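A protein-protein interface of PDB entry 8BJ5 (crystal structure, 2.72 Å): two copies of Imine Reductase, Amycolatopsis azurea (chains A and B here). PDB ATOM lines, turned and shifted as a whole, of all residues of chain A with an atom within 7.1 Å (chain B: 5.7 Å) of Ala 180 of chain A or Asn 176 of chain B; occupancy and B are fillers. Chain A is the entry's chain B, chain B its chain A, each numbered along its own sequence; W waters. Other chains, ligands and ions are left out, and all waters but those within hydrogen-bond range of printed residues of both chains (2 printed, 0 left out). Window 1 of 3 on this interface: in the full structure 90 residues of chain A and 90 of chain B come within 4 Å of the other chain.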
ATOM      1  N   ILE A 173      -5.126  14.330  -7.073  1.00  0.00           N
ATOM      2  CA  ILE A 173      -4.069  13.928  -6.096  1.00  0.00           C
ATOM      3  C   ILE A 173      -3.426  15.177  -5.488  1.00  0.00           C
ATOM      4  O   ILE A 173      -3.214  15.198  -4.255  1.00  0.00           O
ATOM      5  CB  ILE A 173      -2.985  13.051  -6.760  1.00  0.00           C
ATOM      6  CG1 ILE A 173      -3.576  11.740  -7.282  1.00  0.00           C
ATOM      7  CG2 ILE A 173      -1.813  12.825  -5.795  1.00  0.00           C
ATOM      8  CD1 ILE A 173      -2.581  10.837  -7.935  1.00  0.00           C
ATOM      9  N   PHE A 174      -3.070  16.148  -6.329  1.00  0.00           N
ATOM     10  CA  PHE A 174      -2.290  17.356  -5.946  1.00  0.00           C
ATOM     11  C   PHE A 174      -3.060  18.206  -4.924  1.00  0.00           C
ATOM     12  O   PHE A 174      -2.540  18.434  -3.828  1.00  0.00           O
ATOM     13  CB  PHE A 174      -1.938  18.159  -7.200  1.00  0.00           C
ATOM     14  CG  PHE A 174      -1.057  19.344  -6.936  1.00  0.00           C
ATOM     15  CD1 PHE A 174       0.182  19.185  -6.330  1.00  0.00           C
ATOM     16  CD2 PHE A 174      -1.465  20.614  -7.296  1.00  0.00           C
ATOM     17  CE1 PHE A 174       0.991  20.282  -6.070  1.00  0.00           C
ATOM     18  CE2 PHE A 174      -0.660  21.713  -7.037  1.00  0.00           C
ATOM     19  CZ  PHE A 174       0.577  21.541  -6.440  1.00  0.00           C
ATOM     20  N   LEU A 175      -4.255  18.677  -5.292  1.00  0.00           N
ATOM     21  CA  LEU A 175      -5.138  19.463  -4.402  1.00  0.00           C
ATOM     22  C   LEU A 175      -5.379  18.666  -3.120  1.00  0.00           C
ATOM     23  O   LEU A 175      -5.413  19.276  -2.045  1.00  0.00           O
ATOM     24  CB  LEU A 175      -6.467  19.754  -5.096  1.00  0.00           C
ATOM     25  CG  LEU A 175      -6.434  20.683  -6.303  1.00  0.00           C
ATOM     26  CD1 LEU A 175      -7.829  21.229  -6.599  1.00  0.00           C
ATOM     27  CD2 LEU A 175      -5.449  21.812  -6.115  1.00  0.00           C
ATOM     28  N   ASN A 176      -5.557  17.354  -3.227  1.00  0.00           N
ATOM     29  CA  ASN A 176      -5.710  16.455  -2.054  1.00  0.00           C
ATOM     30  C   ASN A 176      -4.468  16.564  -1.176  1.00  0.00           C
ATOM     31  O   ASN A 176      -4.640  16.652   0.048  1.00  0.00           O
ATOM     32  CB  ASN A 176      -5.967  14.998  -2.433  1.00  0.00           C
ATOM     33  CG  ASN A 176      -7.345  14.567  -2.002  1.00  0.00           C
ATOM     34  OD1 ASN A 176      -7.537  14.252  -0.826  1.00  0.00           O
ATOM     35  ND2 ASN A 176      -8.301  14.589  -2.931  1.00  0.00           N
ATOM     36  N   SER A 177      -3.277  16.555  -1.774  1.00  0.00           N
ATOM     37  CA  SER A 177      -1.984  16.514  -1.045  1.00  0.00           C
ATOM     38  C   SER A 177      -1.777  17.847  -0.309  1.00  0.00           C
ATOM     39  O   SER A 177      -1.414  17.834   0.908  1.00  0.00           O
ATOM     40  CB  SER A 177      -0.851  16.156  -1.979  1.00  0.00           C
ATOM     41  OG  SER A 177      -1.077  14.849  -2.498  1.00  0.00           O
ATOM     42  N   LEU A 178      -2.070  18.956  -0.998  1.00  0.00           N
ATOM     43  CA  LEU A 178      -2.044  20.309  -0.391  1.00  0.00           C
ATOM     44  C   LEU A 178      -3.035  20.329   0.781  1.00  0.00           C
ATOM     45  O   LEU A 178      -2.617  20.616   1.894  1.00  0.00           O
ATOM     46  CB  LEU A 178      -2.387  21.364  -1.450  1.00  0.00           C
ATOM     47  CG  LEU A 178      -1.467  21.433  -2.668  1.00  0.00           C
ATOM     48  CD1 LEU A 178      -1.894  22.578  -3.576  1.00  0.00           C
ATOM     49  CD2 LEU A 178       0.003  21.546  -2.259  1.00  0.00           C
ATOM     50  N   SER A 179      -4.297  19.997   0.551  1.00  0.00           N
ATOM     51  CA  SER A 179      -5.332  20.027   1.619  1.00  0.00           C
ATOM     52  C   SER A 179      -4.933  19.084   2.762  1.00  0.00           C
ATOM     53  O   SER A 179      -5.052  19.483   3.918  1.00  0.00           O
ATOM     54  CB  SER A 179      -6.709  19.764   1.091  1.00  0.00           C
ATOM     55  OG  SER A 179      -7.250  20.974   0.564  1.00  0.00           O
ATOM     56  N   ALA A 180      -4.421  17.895   2.471  1.00  0.00           N
ATOM     57  CA  ALA A 180      -4.000  16.932   3.517  1.00  0.00           C
ATOM     58  C   ALA A 180      -2.846  17.551   4.296  1.00  0.00           C
ATOM     59  O   ALA A 180      -2.887  17.525   5.528  1.00  0.00           O
ATOM     60  CB  ALA A 180      -3.602  15.604   2.919  1.00  0.00           C
ATOM     61  N   PHE A 181      -1.870  18.114   3.588  1.00  0.00           N
ATOM     62  CA  PHE A 181      -0.652  18.703   4.196  1.00  0.00           C
ATOM     63  C   PHE A 181      -1.057  19.778   5.204  1.00  0.00           C
ATOM     64  O   PHE A 181      -0.591  19.734   6.354  1.00  0.00           O
ATOM     65  CB  PHE A 181       0.294  19.298   3.156  1.00  0.00           C
ATOM     66  CG  PHE A 181       1.423  20.025   3.835  1.00  0.00           C
ATOM     67  CD1 PHE A 181       2.294  19.343   4.668  1.00  0.00           C
ATOM     68  CD2 PHE A 181       1.540  21.400   3.740  1.00  0.00           C
ATOM     69  CE1 PHE A 181       3.294  20.016   5.351  1.00  0.00           C
ATOM     70  CE2 PHE A 181       2.561  22.063   4.405  1.00  0.00           C
ATOM     71  CZ  PHE A 181       3.427  21.368   5.218  1.00  0.00           C
ATOM     72  N   MET A 182      -1.894  20.710   4.761  1.00  0.00           N
ATOM     73  CA  MET A 182      -2.436  21.826   5.582  1.00  0.00           C
ATOM     74  C   MET A 182      -3.267  21.255   6.735  1.00  0.00           C
ATOM     75  O   MET A 182      -3.117  21.762   7.853  1.00  0.00           O
ATOM     76  CB  MET A 182      -3.274  22.784   4.725  1.00  0.00           C
ATOM     77  CG  MET A 182      -2.388  23.579   3.767  1.00  0.00           C
ATOM     78  SD  MET A 182      -3.219  24.842   2.779  1.00  0.00           S
ATOM     79  CE  MET A 182      -4.157  23.842   1.627  1.00  0.00           C
ATOM     80  N   HIS A 183      -4.055  20.209   6.490  1.00  0.00           N
ATOM     81  CA  HIS A 183      -4.908  19.567   7.525  1.00  0.00           C
ATOM     82  C   HIS A 183      -4.030  18.980   8.637  1.00  0.00           C
ATOM     83  O   HIS A 183      -4.288  19.294   9.817  1.00  0.00           O
ATOM     84  CB  HIS A 183      -5.866  18.541   6.908  1.00  0.00           C
ATOM     85  CG  HIS A 183      -6.869  18.036   7.884  1.00  0.00           C
ATOM     86  ND1 HIS A 183      -6.570  17.071   8.805  1.00  0.00           N
ATOM     87  CD2 HIS A 183      -8.145  18.397   8.116  1.00  0.00           C
ATOM     88  CE1 HIS A 183      -7.615  16.843   9.563  1.00  0.00           C
ATOM     89  NE2 HIS A 183      -8.599  17.635   9.153  1.00  0.00           N
ATOM     90  N   ALA A 184      -3.007  18.200   8.280  1.00  0.00           N
ATOM     91  CA  ALA A 184      -2.055  17.558   9.225  1.00  0.00           C
ATOM     92  C   ALA A 184      -1.310  18.643  10.009  1.00  0.00           C
ATOM     93  O   ALA A 184      -1.160  18.520  11.232  1.00  0.00           O
ATOM     94  CB  ALA A 184      -1.088  16.681   8.465  1.00  0.00           C
ATOM     95  N   SER A 185      -0.858  19.675   9.301  1.00  0.00           N
ATOM     96  CA  SER A 185      -0.158  20.848   9.870  1.00  0.00           C
ATOM     97  C   SER A 185      -1.079  21.516  10.896  1.00  0.00           C
ATOM     98  O   SER A 185      -0.595  21.823  12.009  1.00  0.00           O
ATOM     99  CB  SER A 185       0.297  21.775   8.766  1.00  0.00           C
ATOM    100  OG  SER A 185       1.217  21.104   7.890  1.00  0.00           O
ATOM    101  N   ALA A 186      -2.361  21.691  10.547  1.00  0.00           N
ATOM    102  CA  ALA A 186      -3.401  22.307  11.405  1.00  0.00           C
ATOM    103  C   ALA A 186      -3.574  21.482  12.681  1.00  0.00           C
ATOM    104  O   ALA A 186      -3.844  22.077  13.745  1.00  0.00           O
ATOM    105  CB  ALA A 186      -4.698  22.425  10.646  1.00  0.00           C
ATOM    106  N   PHE A 198       7.432  19.673  11.826  1.00  0.00           N
ATOM    107  CA  PHE A 198       6.638  18.587  11.191  1.00  0.00           C
ATOM    108  C   PHE A 198       6.946  18.518   9.693  1.00  0.00           C
ATOM    109  O   PHE A 198       6.982  17.381   9.202  1.00  0.00           O
ATOM    110  CB  PHE A 198       5.136  18.755  11.457  1.00  0.00           C
ATOM    111  CG  PHE A 198       4.280  17.764  10.712  1.00  0.00           C
ATOM    112  CD1 PHE A 198       4.379  16.410  10.975  1.00  0.00           C
ATOM    113  CD2 PHE A 198       3.392  18.185   9.739  1.00  0.00           C
ATOM    114  CE1 PHE A 198       3.612  15.493  10.275  1.00  0.00           C
ATOM    115  CE2 PHE A 198       2.629  17.267   9.031  1.00  0.00           C
ATOM    116  CZ  PHE A 198       2.738  15.922   9.306  1.00  0.00           C
ATOM    117  N   PHE A 206       5.486  12.110   1.584  1.00  0.00           N
ATOM    118  CA  PHE A 206       5.134  12.276   0.147  1.00  0.00           C
ATOM    119  C   PHE A 206       6.196  11.634  -0.760  1.00  0.00           C
ATOM    120  O   PHE A 206       5.815  10.995  -1.760  1.00  0.00           O
ATOM    121  CB  PHE A 206       4.959  13.760  -0.200  1.00  0.00           C
ATOM    122  CG  PHE A 206       3.671  14.382   0.286  1.00  0.00           C
ATOM    123  CD1 PHE A 206       2.471  14.007  -0.288  1.00  0.00           C
ATOM    124  CD2 PHE A 206       3.653  15.378   1.255  1.00  0.00           C
ATOM    125  CE1 PHE A 206       1.277  14.572   0.127  1.00  0.00           C
ATOM    126  CE2 PHE A 206       2.455  15.916   1.691  1.00  0.00           C
ATOM    127  CZ  PHE A 206       1.268  15.521   1.119  1.00  0.00           C
ATOM    128  N   ILE A 242      -7.883   9.772  13.123  1.00  0.00           N
ATOM    129  CA  ILE A 242      -7.583  11.095  12.498  1.00  0.00           C
ATOM    130  C   ILE A 242      -8.842  11.968  12.596  1.00  0.00           C
ATOM    131  O   ILE A 242      -8.716  13.168  12.938  1.00  0.00           O
ATOM    132  CB  ILE A 242      -7.115  10.972  11.033  1.00  0.00           C
ATOM    133  CG1 ILE A 242      -5.862  10.117  10.881  1.00  0.00           C
ATOM    134  CG2 ILE A 242      -6.909  12.350  10.419  1.00  0.00           C
ATOM    135  CD1 ILE A 242      -5.787   9.420   9.547  1.00  0.00           C
ATOM    136  N   LEU A 255     -12.236  16.536   5.271  1.00  0.00           N
ATOM    137  CA  LEU A 255     -11.245  15.732   4.527  1.00  0.00           C
ATOM    138  C   LEU A 255     -11.029  14.379   5.199  1.00  0.00           C
ATOM    139  O   LEU A 255     -11.096  13.354   4.529  1.00  0.00           O
ATOM    140  CB  LEU A 255      -9.937  16.502   4.354  1.00  0.00           C
ATOM    141  CG  LEU A 255      -9.073  15.937   3.220  1.00  0.00           C
ATOM    142  CD1 LEU A 255      -9.567  16.409   1.851  1.00  0.00           C
ATOM    143  CD2 LEU A 255      -7.616  16.305   3.438  1.00  0.00           C
ATOM    144  N   PRO A 256     -10.777  14.295   6.520  1.00  0.00           N
ATOM    145  CA  PRO A 256     -10.635  12.992   7.177  1.00  0.00           C
ATOM    146  C   PRO A 256     -11.934  12.163   7.208  1.00  0.00           C
ATOM    147  O   PRO A 256     -11.833  10.943   7.177  1.00  0.00           O
ATOM    148  CB  PRO A 256     -10.184  13.338   8.602  1.00  0.00           C
ATOM    149  CG  PRO A 256     -10.739  14.730   8.810  1.00  0.00           C
ATOM    150  CD  PRO A 256     -10.592  15.411   7.460  1.00  0.00           C
ATOM    151  N   ALA A 258     -14.136  12.162   4.774  1.00  0.00           N
ATOM    152  CA  ALA A 258     -14.167  11.614   3.397  1.00  0.00           C
ATOM    153  C   ALA A 258     -13.253  10.383   3.317  1.00  0.00           C
ATOM    154  O   ALA A 258     -13.690   9.371   2.749  1.00  0.00           O
ATOM    155  CB  ALA A 258     -13.788  12.670   2.387  1.00  0.00           C
ATOM    156  N   VAL A 259     -12.042  10.441   3.877  1.00  0.00           N
ATOM    157  CA  VAL A 259     -11.127   9.260   3.893  1.00  0.00           C
ATOM    158  C   VAL A 259     -11.791   8.148   4.715  1.00  0.00           C
ATOM    159  O   VAL A 259     -11.870   7.025   4.210  1.00  0.00           O
ATOM    160  CB  VAL A 259      -9.713   9.631   4.388  1.00  0.00           C
ATOM    161  CG1 VAL A 259      -8.937   8.435   4.940  1.00  0.00           C
ATOM    162  CG2 VAL A 259      -8.929  10.323   3.275  1.00  0.00           C
ATOM    163  N   HIS A 262     -14.435   6.093   2.767  1.00  0.00           N
ATOM    164  CA  HIS A 262     -13.842   5.025   1.923  1.00  0.00           C
ATOM    165  C   HIS A 262     -13.705   3.749   2.764  1.00  0.00           C
ATOM    166  O   HIS A 262     -14.215   2.689   2.329  1.00  0.00           O
ATOM    167  CB  HIS A 262     -12.497   5.465   1.341  1.00  0.00           C
ATOM    168  CG  HIS A 262     -12.602   6.512   0.289  1.00  0.00           C
ATOM    169  ND1 HIS A 262     -11.496   7.208  -0.154  1.00  0.00           N
ATOM    170  CD2 HIS A 262     -13.673   7.022  -0.353  1.00  0.00           C
ATOM    171  CE1 HIS A 262     -11.876   8.079  -1.060  1.00  0.00           C
ATOM    172  NE2 HIS A 262     -13.204   7.966  -1.214  1.00  0.00           N
ATOM    173  N   TYR A 263     -13.067   3.843   3.934  1.00  0.00           N
ATOM    174  CA  TYR A 263     -12.855   2.678   4.822  1.00  0.00           C
ATOM    175  C   TYR A 263     -14.223   2.134   5.260  1.00  0.00           C
ATOM    176  O   TYR A 263     -14.447   0.907   5.177  1.00  0.00           O
ATOM    177  CB  TYR A 263     -11.873   3.039   5.936  1.00  0.00           C
ATOM    178  CG  TYR A 263     -10.481   3.181   5.385  1.00  0.00           C
ATOM    179  CD1 TYR A 263      -9.640   2.087   5.271  1.00  0.00           C
ATOM    180  CD2 TYR A 263     -10.026   4.389   4.890  1.00  0.00           C
ATOM    181  CE1 TYR A 263      -8.371   2.190   4.720  1.00  0.00           C
ATOM    182  CE2 TYR A 263      -8.767   4.510   4.321  1.00  0.00           C
ATOM    183  CZ  TYR A 263      -7.935   3.405   4.233  1.00  0.00           C
ATOM    184  OH  TYR A 263      -6.695   3.513   3.673  1.00  0.00           O
ATOM    185  N   LEU B 171      -0.394   9.915   9.083  1.00  0.00           N
ATOM    186  CA  LEU B 171      -1.424   9.037   8.483  1.00  0.00           C
ATOM    187  C   LEU B 171      -2.528   9.895   7.864  1.00  0.00           C
ATOM    188  O   LEU B 171      -3.082   9.464   6.845  1.00  0.00           O
ATOM    189  CB  LEU B 171      -1.916   8.044   9.534  1.00  0.00           C
ATOM    190  CG  LEU B 171      -1.101   6.735   9.520  1.00  0.00           C
ATOM    191  CD1 LEU B 171       0.306   6.920  10.082  1.00  0.00           C
ATOM    192  CD2 LEU B 171      -1.838   5.624  10.231  1.00  0.00           C
ATOM    193  N   ASP B 172      -2.780  11.084   8.409  1.00  0.00           N
ATOM    194  CA  ASP B 172      -3.698  12.091   7.813  1.00  0.00           C
ATOM    195  C   ASP B 172      -3.311  12.276   6.337  1.00  0.00           C
ATOM    196  O   ASP B 172      -4.206  12.083   5.475  1.00  0.00           O
ATOM    197  CB  ASP B 172      -3.651  13.382   8.633  1.00  0.00           C
ATOM    198  CG  ASP B 172      -4.620  14.481   8.250  1.00  0.00           C
ATOM    199  OD1 ASP B 172      -5.389  14.285   7.265  1.00  0.00           O
ATOM    200  OD2 ASP B 172      -4.575  15.529   8.946  1.00  0.00           O
ATOM    201  N   ILE B 173      -2.027  12.579   6.062  1.00  0.00           N
ATOM    202  CA  ILE B 173      -1.463  12.783   4.692  1.00  0.00           C
ATOM    203  C   ILE B 173      -1.477  11.455   3.930  1.00  0.00           C
ATOM    204  O   ILE B 173      -1.893  11.458   2.736  1.00  0.00           O
ATOM    205  CB  ILE B 173      -0.030  13.334   4.741  1.00  0.00           C
ATOM    206  CG1 ILE B 173       0.024  14.717   5.388  1.00  0.00           C
ATOM    207  CG2 ILE B 173       0.608  13.326   3.352  1.00  0.00           C
ATOM    208  CD1 ILE B 173       1.431  15.197   5.635  1.00  0.00           C
ATOM    209  N   PHE B 174      -0.993  10.387   4.575  1.00  0.00           N
ATOM    210  CA  PHE B 174      -0.776   9.060   3.950  1.00  0.00           C
ATOM    211  C   PHE B 174      -2.106   8.470   3.441  1.00  0.00           C
ATOM    212  O   PHE B 174      -2.212   8.184   2.235  1.00  0.00           O
ATOM    213  CB  PHE B 174      -0.124   8.104   4.944  1.00  0.00           C
ATOM    214  CG  PHE B 174       0.268   6.787   4.339  1.00  0.00           C
ATOM    215  CD1 PHE B 174       1.138   6.740   3.264  1.00  0.00           C
ATOM    216  CD2 PHE B 174      -0.213   5.601   4.853  1.00  0.00           C
ATOM    217  CE1 PHE B 174       1.542   5.528   2.717  1.00  0.00           C
ATOM    218  CE2 PHE B 174       0.188   4.385   4.310  1.00  0.00           C
ATOM    219  CZ  PHE B 174       1.054   4.352   3.233  1.00  0.00           C
ATOM    220  N   LEU B 175      -3.072   8.263   4.340  1.00  0.00           N
ATOM    221  CA  LEU B 175      -4.387   7.688   4.003  1.00  0.00           C
ATOM    222  C   LEU B 175      -5.042   8.591   2.961  1.00  0.00           C
ATOM    223  O   LEU B 175      -5.718   8.042   2.057  1.00  0.00           O
ATOM    224  CB  LEU B 175      -5.253   7.606   5.260  1.00  0.00           C
ATOM    225  CG  LEU B 175      -4.806   6.625   6.340  1.00  0.00           C
ATOM    226  CD1 LEU B 175      -5.946   6.360   7.325  1.00  0.00           C
ATOM    227  CD2 LEU B 175      -4.312   5.330   5.725  1.00  0.00           C
ATOM    228  N   ASN B 176      -4.861   9.917   3.078  1.00  0.00           N
ATOM    229  CA  ASN B 176      -5.354  10.871   2.049  1.00  0.00           C
ATOM    230  C   ASN B 176      -4.727  10.533   0.694  1.00  0.00           C
ATOM    231  O   ASN B 176      -5.453  10.538  -0.296  1.00  0.00           O
ATOM    232  CB  ASN B 176      -5.089  12.332   2.407  1.00  0.00           C
ATOM    233  CG  ASN B 176      -6.383  13.075   2.637  1.00  0.00           C
ATOM    234  OD1 ASN B 176      -7.081  13.420   1.686  1.00  0.00           O
ATOM    235  ND2 ASN B 176      -6.739  13.271   3.896  1.00  0.00           N
ATOM    236  N   SER B 177      -3.420  10.265   0.661  1.00  0.00           N
ATOM    237  CA  SER B 177      -2.643  10.070  -0.587  1.00  0.00           C
ATOM    238  C   SER B 177      -3.056   8.746  -1.237  1.00  0.00           C
ATOM    239  O   SER B 177      -3.285   8.726  -2.480  1.00  0.00           O
ATOM    240  CB  SER B 177      -1.172  10.183  -0.305  1.00  0.00           C
ATOM    241  OG  SER B 177      -0.878  11.504   0.174  1.00  0.00           O
ATOM    242  N   LEU B 178      -3.236   7.702  -0.424  1.00  0.00           N
ATOM    243  CA  LEU B 178      -3.782   6.398  -0.883  1.00  0.00           C
ATOM    244  C   LEU B 178      -5.164   6.660  -1.490  1.00  0.00           C
ATOM    245  O   LEU B 178      -5.355   6.355  -2.672  1.00  0.00           O
ATOM    246  CB  LEU B 178      -3.847   5.392   0.274  1.00  0.00           C
ATOM    247  CG  LEU B 178      -2.504   5.050   0.937  1.00  0.00           C
ATOM    248  CD1 LEU B 178      -2.654   3.920   1.938  1.00  0.00           C
ATOM    249  CD2 LEU B 178      -1.402   4.712  -0.068  1.00  0.00           C
ATOM    250  N   SER B 179      -6.087   7.235  -0.724  1.00  0.00           N
ATOM    251  CA  SER B 179      -7.471   7.480  -1.207  1.00  0.00           C
ATOM    252  C   SER B 179      -7.434   8.361  -2.467  1.00  0.00           C
ATOM    253  O   SER B 179      -8.153   8.040  -3.430  1.00  0.00           O
ATOM    254  CB  SER B 179      -8.359   8.037  -0.134  1.00  0.00           C
ATOM    255  OG  SER B 179      -8.901   6.966   0.620  1.00  0.00           O
ATOM    256  N   ALA B 180      -6.612   9.411  -2.492  1.00  0.00           N
ATOM    257  CA  ALA B 180      -6.514  10.312  -3.663  1.00  0.00           C
ATOM    258  C   ALA B 180      -6.009   9.502  -4.861  1.00  0.00           C
ATOM    259  O   ALA B 180      -6.614   9.592  -5.942  1.00  0.00           O
ATOM    260  CB  ALA B 180      -5.622  11.487  -3.376  1.00  0.00           C
ATOM    261  N   PHE B 181      -4.958   8.705  -4.651  1.00  0.00           N
ATOM    262  CA  PHE B 181      -4.316   7.901  -5.716  1.00  0.00           C
ATOM    263  C   PHE B 181      -5.365   6.997  -6.366  1.00  0.00           C
ATOM    264  O   PHE B 181      -5.473   7.001  -7.608  1.00  0.00           O
ATOM    265  CB  PHE B 181      -3.159   7.050  -5.186  1.00  0.00           C
ATOM    266  CG  PHE B 181      -2.674   6.089  -6.238  1.00  0.00           C
ATOM    267  CD1 PHE B 181      -2.136   6.580  -7.420  1.00  0.00           C
ATOM    268  CD2 PHE B 181      -2.863   4.725  -6.106  1.00  0.00           C
ATOM    269  CE1 PHE B 181      -1.742   5.718  -8.430  1.00  0.00           C
ATOM    270  CE2 PHE B 181      -2.468   3.870  -7.122  1.00  0.00           C
ATOM    271  CZ  PHE B 181      -1.912   4.366  -8.279  1.00  0.00           C
ATOM    272  N   LEU B 255     -14.471  12.516  -1.507  1.00  0.00           N
ATOM    273  CA  LEU B 255     -13.096  13.047  -1.326  1.00  0.00           C
ATOM    274  C   LEU B 255     -12.940  14.352  -2.104  1.00  0.00           C
ATOM    275  O   LEU B 255     -12.465  15.328  -1.538  1.00  0.00           O
ATOM    276  CB  LEU B 255     -12.058  11.999  -1.731  1.00  0.00           C
ATOM    277  CG  LEU B 255     -10.651  12.306  -1.220  1.00  0.00           C
ATOM    278  CD1 LEU B 255     -10.516  11.945   0.256  1.00  0.00           C
ATOM    279  CD2 LEU B 255      -9.591  11.597  -2.051  1.00  0.00           C
HETATM  280  O   HOH W   1      -3.551  13.342   0.026  1.00  0.00           O
HETATM  281  O   HOH W   2      -7.080   5.600   2.057  1.00  0.00           O
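OD2 of Asp 172 of chain B sits at hydrogen-bond distance from N of Ala 184 of chain A (3.2 Å).
The side-chain amide oxygen (OD1) of Asn 176 of chain B sits close to the side-chain amide oxygen (OD1) of Asn 176 of chain A, 2.7 Å away.
OG of Ser 179 of chain B is in hydrogen-bond range of ND1 of His 262 of chain A (2.7 Å).
OD2 of Asp 172 of chain B lies within hydrogen-bond range of ND1 of His 183 of chain A, at 2.5 Å.
O of Ile 173 of chain A is in hydrogen-bond range of OG of Ser 177 of chain A.
O of Asp 172 of chain B lies close to ND2 of Asn 176 of chain B, 3.2 Å away.
The side-chain hydroxyl (OG) of Ser 177 of chain B is in hydrogen-bond range of the backbone carbonyl oxygen (O) of Ile 173 of chain B, 2.8 Å away.
Among the printed residues, merely in contact across the chains: Ile 173 of chain A with Ala 180 of chain B, Asn 176 of chain A with Ala 180 of chain B, Asn 176 of chain A with Leu 255 of chain B, Ala 180 of chain A with Ile 173 of chain B, Ala 180 of chain A with Asn 176 of chain B, Ala 184 of chain A with Ile 173 of chain B, Phe 198 of chain A with Ile 173 of chain B, Phe 206 of chain A with Ile 173 of chain B, Phe 206 of chain A with Ser 177 of chain B, Ile 242 of chain A with Leu 171 of chain B, Ile 242 of chain A with Asp 172 of chain B, Ile 242 of chain A with Leu 175 of chain B, Leu 255 of chain A with Asn 176 of chain B, Ala 258 of chain A with Leu 255 of chain B, Val 259 of chain A with Leu 175 of chain B, Val 259 of chain A with Asn 176 of chain B, Val 259 of chain A with Leu 255 of chain B, His 262 of chain A with Leu 255 of chain B and Tyr 263 of chain A with Leu 175 of chain B.
Printed residues of chain B within 4 Å of Ala 180 of chain A: Ile 173 and Asn 176.
Of the printed residues of chain B, Ile 173 of chain A touches Ala 180.
Of the printed residues of chain A, Ala 180 of chain B touches Ile 173 (3.95 Å) and Asn 176 (3.7 Å).
Leu 178 of chain A touches none of the printed residues of chain B.
Ser 177 of chain A touches none of the printed residues of chain B.
The nearest residue of chain B that does not touch Ala 180 of chain A is Asp 172 of chain B (4.3 Å).
The nearest residue of chain A that does not touch Asn 176 of chain B is Pro 256 of chain A (4.9 Å).
Of the 23 printed residues of chain A, 13 touch a printed residue of chain B.
Hydrophobic or aromatic side chains of chain A that line the printed part of chain B: Ile 173, Ala 180, His 183, Ala 184, Phe 198, Phe 206, Ile 242, Leu 255, Ala 258, Val 259, His 262 and Tyr 263.
Of the 12 printed residues of chain B, 9 touch a printed residue of chain A.
Ile 173 of chain A touches Ala 180 of chain B, and with the chains exchanged Ala 180 of chain A touches Ile 173 of chain B.
Asn 176 of chain B touches its own counterpart, Asn 176 of chain A.
Asn 176 of chain A touches Ala 180 of chain B, and with the chains exchanged Ala 180 of chain A touches Asn 176 of chain B.
Asn 176 of chain A touches Leu 255 of chain B, and with the chains exchanged Leu 255 of chain A touches Asn 176 of chain B.
10 positions are printed for both chains.
Water W2 lies within hydrogen-bond range of the side-chain hydroxyl (OH) of Tyr 263 of chain A (2.7 Å), the side-chain hydroxyl (OG) of Ser 179 of chain B (2.7 Å) and the backbone carbonyl oxygen (O) of Leu 175 of chain B (2.8 Å).
Water W1 lies within hydrogen-bond range of N of Ser 177 of chain B (3.1 Å), O of Asn 176 of chain B (3.4 Å) and O of Asn 176 of chain A (3.5 Å).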
